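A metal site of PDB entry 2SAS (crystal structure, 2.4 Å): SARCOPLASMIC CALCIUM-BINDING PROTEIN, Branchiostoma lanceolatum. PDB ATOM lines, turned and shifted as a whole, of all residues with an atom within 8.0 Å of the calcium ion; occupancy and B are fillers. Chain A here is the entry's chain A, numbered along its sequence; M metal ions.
The calcium ion is bound by OD1 of Asp 115. OE1 of Glu 126 binds the calcium ion (2.2 Å). The calcium ion is bound by OD1 of Asp 119 (2.3 Å). The backbone carbonyl oxygen (O) of Ile 121 binds the calcium ion, 2.4 Å away. The calcium ion is bound by OG of Ser 117. OE2 of Glu 126 binds the calcium ion (2.5 Å).
The side-chain carboxylate (OE2) of Glu 126 sits close to the backbone NH (N) of Val 116, at 3.5 Å. The backbone NH (N) of Gly 120 is in hydrogen-bond range of the side-chain carboxylate (OD2) of Asp 115 (2.6 Å). The side-chain carboxylate (OD1) of Asp 123 lies within hydrogen-bond range of the backbone NH (N) of Glu 126 (3.1 Å). OD1 of Asp 115 lies close to N of Gly 118 (3.0 Å).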
ATOM      1  N   PHE A 111      12.890 -10.376 -19.051  1.00  0.00           N
ATOM      2  CA  PHE A 111      12.677  -8.953 -18.745  1.00  0.00           C
ATOM      3  C   PHE A 111      13.966  -8.143 -18.720  1.00  0.00           C
ATOM      4  O   PHE A 111      13.961  -7.063 -19.335  1.00  0.00           O
ATOM      5  CB  PHE A 111      11.907  -8.709 -17.483  1.00  0.00           C
ATOM      6  CG  PHE A 111      11.655  -7.243 -17.179  1.00  0.00           C
ATOM      7  CD1 PHE A 111      10.638  -6.574 -17.861  1.00  0.00           C
ATOM      8  CD2 PHE A 111      12.369  -6.610 -16.143  1.00  0.00           C
ATOM      9  CE1 PHE A 111      10.358  -5.247 -17.567  1.00  0.00           C
ATOM     10  CE2 PHE A 111      12.052  -5.294 -15.816  1.00  0.00           C
ATOM     11  CZ  PHE A 111      11.072  -4.593 -16.539  1.00  0.00           C
ATOM     12  N   LYS A 112      14.994  -8.602 -18.040  1.00  0.00           N
ATOM     13  CA  LYS A 112      16.279  -7.902 -17.903  1.00  0.00           C
ATOM     14  C   LYS A 112      17.031  -7.789 -19.211  1.00  0.00           C
ATOM     15  O   LYS A 112      17.944  -6.955 -19.327  1.00  0.00           O
ATOM     16  CB  LYS A 112      17.206  -8.613 -16.923  1.00  0.00           C
ATOM     17  CG  LYS A 112      16.931  -8.354 -15.458  1.00  0.00           C
ATOM     18  CD  LYS A 112      17.338  -9.558 -14.602  1.00  0.00           C
ATOM     19  CE  LYS A 112      16.701  -9.481 -13.238  1.00  0.00           C
ATOM     20  NZ  LYS A 112      17.326 -10.396 -12.257  1.00  0.00           N
ATOM     21  N   MET A 114      15.494  -7.057 -21.873  1.00  0.00           N
ATOM     22  CA  MET A 114      14.686  -6.040 -22.635  1.00  0.00           C
ATOM     23  C   MET A 114      15.074  -4.676 -22.042  1.00  0.00           C
ATOM     24  O   MET A 114      15.412  -3.736 -22.776  1.00  0.00           O
ATOM     25  CB  MET A 114      13.228  -6.357 -22.566  1.00  0.00           C
ATOM     26  CG  MET A 114      12.780  -7.418 -23.478  1.00  0.00           C
ATOM     27  SD  MET A 114      11.129  -7.986 -22.939  1.00  0.00           S
ATOM     28  CE  MET A 114      10.142  -6.653 -23.632  1.00  0.00           C
ATOM     29  N   ASP A 115      15.075  -4.641 -20.727  1.00  0.00           N
ATOM     30  CA  ASP A 115      15.440  -3.428 -20.004  1.00  0.00           C
ATOM     31  C   ASP A 115      16.934  -3.176 -20.163  1.00  0.00           C
ATOM     32  O   ASP A 115      17.681  -3.234 -19.175  1.00  0.00           O
ATOM     33  CB  ASP A 115      14.963  -3.568 -18.556  1.00  0.00           C
ATOM     34  CG  ASP A 115      15.348  -2.520 -17.568  1.00  0.00           C
ATOM     35  OD1 ASP A 115      15.689  -1.364 -17.899  1.00  0.00           O
ATOM     36  OD2 ASP A 115      15.271  -2.854 -16.350  1.00  0.00           O
ATOM     37  N   VAL A 116      17.426  -2.877 -21.357  1.00  0.00           N
ATOM     38  CA  VAL A 116      18.846  -2.597 -21.566  1.00  0.00           C
ATOM     39  C   VAL A 116      19.440  -1.559 -20.601  1.00  0.00           C
ATOM     40  O   VAL A 116      20.687  -1.583 -20.316  1.00  0.00           O
ATOM     41  CB  VAL A 116      19.029  -2.205 -23.052  1.00  0.00           C
ATOM     42  CG1 VAL A 116      20.349  -1.445 -23.277  1.00  0.00           C
ATOM     43  CG2 VAL A 116      18.925  -3.416 -23.972  1.00  0.00           C
ATOM     44  N   SER A 117      18.624  -0.645 -20.059  1.00  0.00           N
ATOM     45  CA  SER A 117      19.149   0.394 -19.177  1.00  0.00           C
ATOM     46  C   SER A 117      19.202   0.100 -17.696  1.00  0.00           C
ATOM     47  O   SER A 117      19.792   0.969 -16.978  1.00  0.00           O
ATOM     48  CB  SER A 117      18.378   1.697 -19.330  1.00  0.00           C
ATOM     49  OG  SER A 117      17.120   1.562 -18.700  1.00  0.00           O
ATOM     50  N   GLY A 118      18.605  -0.958 -17.169  1.00  0.00           N
ATOM     51  CA  GLY A 118      18.703  -1.230 -15.740  1.00  0.00           C
ATOM     52  C   GLY A 118      17.810  -0.518 -14.795  1.00  0.00           C
ATOM     53  O   GLY A 118      17.938  -0.774 -13.570  1.00  0.00           O
ATOM     54  N   ASP A 119      16.880   0.302 -15.189  1.00  0.00           N
ATOM     55  CA  ASP A 119      15.950   1.000 -14.302  1.00  0.00           C
ATOM     56  C   ASP A 119      14.750   0.163 -13.956  1.00  0.00           C
ATOM     57  O   ASP A 119      13.931   0.631 -13.152  1.00  0.00           O
ATOM     58  CB  ASP A 119      15.474   2.361 -14.834  1.00  0.00           C
ATOM     59  CG  ASP A 119      14.987   2.409 -16.223  1.00  0.00           C
ATOM     60  OD1 ASP A 119      14.957   1.435 -17.018  1.00  0.00           O
ATOM     61  OD2 ASP A 119      14.589   3.516 -16.665  1.00  0.00           O
ATOM     62  N   GLY A 120      14.610  -1.013 -14.566  1.00  0.00           N
ATOM     63  CA  GLY A 120      13.414  -1.844 -14.179  1.00  0.00           C
ATOM     64  C   GLY A 120      12.154  -1.392 -14.866  1.00  0.00           C
ATOM     65  O   GLY A 120      11.061  -1.617 -14.352  1.00  0.00           O
ATOM     66  N   ILE A 121      12.295  -0.747 -16.001  1.00  0.00           N
ATOM     67  CA  ILE A 121      11.166  -0.251 -16.809  1.00  0.00           C
ATOM     68  C   ILE A 121      11.583  -0.572 -18.234  1.00  0.00           C
ATOM     69  O   ILE A 121      12.788  -0.325 -18.374  1.00  0.00           O
ATOM     70  CB  ILE A 121      11.024   1.311 -16.649  1.00  0.00           C
ATOM     71  CG1 ILE A 121      10.474   1.599 -15.223  1.00  0.00           C
ATOM     72  CG2 ILE A 121      10.207   2.036 -17.739  1.00  0.00           C
ATOM     73  CD1 ILE A 121      10.551   3.093 -14.879  1.00  0.00           C
ATOM     74  N   VAL A 122      10.770  -1.060 -19.136  1.00  0.00           N
ATOM     75  CA  VAL A 122      11.344  -1.194 -20.499  1.00  0.00           C
ATOM     76  C   VAL A 122      10.605   0.011 -21.159  1.00  0.00           C
ATOM     77  O   VAL A 122       9.347   0.011 -21.152  1.00  0.00           O
ATOM     78  CB  VAL A 122      11.313  -2.535 -21.237  1.00  0.00           C
ATOM     79  CG1 VAL A 122      11.101  -3.728 -20.337  1.00  0.00           C
ATOM     80  CG2 VAL A 122      10.494  -2.580 -22.490  1.00  0.00           C
ATOM     81  N   ASP A 123      11.411   0.978 -21.575  1.00  0.00           N
ATOM     82  CA  ASP A 123      10.741   2.172 -22.152  1.00  0.00           C
ATOM     83  C   ASP A 123      10.499   1.842 -23.622  1.00  0.00           C
ATOM     84  O   ASP A 123      10.905   0.701 -23.942  1.00  0.00           O
ATOM     85  CB  ASP A 123      11.523   3.432 -21.892  1.00  0.00           C
ATOM     86  CG  ASP A 123      12.918   3.419 -22.399  1.00  0.00           C
ATOM     87  OD1 ASP A 123      13.193   2.967 -23.499  1.00  0.00           O
ATOM     88  OD2 ASP A 123      13.823   3.856 -21.653  1.00  0.00           O
ATOM     89  N   LEU A 124       9.923   2.761 -24.336  1.00  0.00           N
ATOM     90  CA  LEU A 124       9.595   2.643 -25.757  1.00  0.00           C
ATOM     91  C   LEU A 124      10.796   2.321 -26.636  1.00  0.00           C
ATOM     92  O   LEU A 124      10.700   1.512 -27.560  1.00  0.00           O
ATOM     93  CB  LEU A 124       8.919   3.963 -26.160  1.00  0.00           C
ATOM     94  CG  LEU A 124       7.775   4.082 -27.133  1.00  0.00           C
ATOM     95  CD1 LEU A 124       7.926   5.429 -27.911  1.00  0.00           C
ATOM     96  CD2 LEU A 124       7.796   2.963 -28.148  1.00  0.00           C
ATOM     97  N   GLU A 125      11.934   2.964 -26.440  1.00  0.00           N
ATOM     98  CA  GLU A 125      13.113   2.698 -27.261  1.00  0.00           C
ATOM     99  C   GLU A 125      13.617   1.281 -27.011  1.00  0.00           C
ATOM    100  O   GLU A 125      13.986   0.590 -27.971  1.00  0.00           O
ATOM    101  CB  GLU A 125      14.181   3.723 -27.133  1.00  0.00           C
ATOM    102  CG  GLU A 125      15.676   3.410 -27.042  1.00  0.00           C
ATOM    103  CD  GLU A 125      16.227   3.639 -25.653  1.00  0.00           C
ATOM    104  OE1 GLU A 125      15.924   4.784 -25.213  1.00  0.00           O
ATOM    105  OE2 GLU A 125      16.860   2.803 -25.008  1.00  0.00           O
ATOM    106  N   GLU A 126      13.551   0.892 -25.748  1.00  0.00           N
ATOM    107  CA  GLU A 126      13.969  -0.491 -25.375  1.00  0.00           C
ATOM    108  C   GLU A 126      13.037  -1.477 -26.038  1.00  0.00           C
ATOM    109  O   GLU A 126      13.477  -2.461 -26.680  1.00  0.00           O
ATOM    110  CB  GLU A 126      13.952  -0.675 -23.846  1.00  0.00           C
ATOM    111  CG  GLU A 126      14.916   0.317 -23.165  1.00  0.00           C
ATOM    112  CD  GLU A 126      15.116   0.261 -21.737  1.00  0.00           C
ATOM    113  OE1 GLU A 126      14.104   0.045 -21.028  1.00  0.00           O
ATOM    114  OE2 GLU A 126      16.199   0.371 -21.160  1.00  0.00           O
ATOM    115  N   PHE A 127      11.740  -1.169 -25.968  1.00  0.00           N
ATOM    116  CA  PHE A 127      10.719  -2.033 -26.581  1.00  0.00           C
ATOM    117  C   PHE A 127      11.010  -2.131 -28.063  1.00  0.00           C
ATOM    118  O   PHE A 127      11.008  -3.247 -28.632  1.00  0.00           O
ATOM    119  CB  PHE A 127       9.290  -1.616 -26.184  1.00  0.00           C
ATOM    120  CG  PHE A 127       8.284  -2.540 -26.814  1.00  0.00           C
ATOM    121  CD1 PHE A 127       8.122  -3.826 -26.262  1.00  0.00           C
ATOM    122  CD2 PHE A 127       7.577  -2.158 -27.958  1.00  0.00           C
ATOM    123  CE1 PHE A 127       7.282  -4.764 -26.839  1.00  0.00           C
ATOM    124  CE2 PHE A 127       6.687  -3.063 -28.538  1.00  0.00           C
ATOM    125  CZ  PHE A 127       6.556  -4.372 -27.970  1.00  0.00           C
ATOM    126  N   PHE A 156       5.568  -0.285 -17.655  1.00  0.00           N
ATOM    127  CA  PHE A 156       6.107  -1.484 -18.206  1.00  0.00           C
ATOM    128  C   PHE A 156       7.262  -1.932 -17.275  1.00  0.00           C
ATOM    129  O   PHE A 156       8.437  -1.729 -17.588  1.00  0.00           O
ATOM    130  CB  PHE A 156       6.568  -1.462 -19.664  1.00  0.00           C
ATOM    131  CG  PHE A 156       6.745  -2.800 -20.342  1.00  0.00           C
ATOM    132  CD1 PHE A 156       6.530  -3.993 -19.664  1.00  0.00           C
ATOM    133  CD2 PHE A 156       7.114  -2.823 -21.694  1.00  0.00           C
ATOM    134  CE1 PHE A 156       6.676  -5.233 -20.300  1.00  0.00           C
ATOM    135  CE2 PHE A 156       7.310  -4.064 -22.335  1.00  0.00           C
ATOM    136  CZ  PHE A 156       7.095  -5.280 -21.639  1.00  0.00           C
HETATM  137 CA    CA M   1      14.988   0.413 -19.024  1.00  0.00          CA
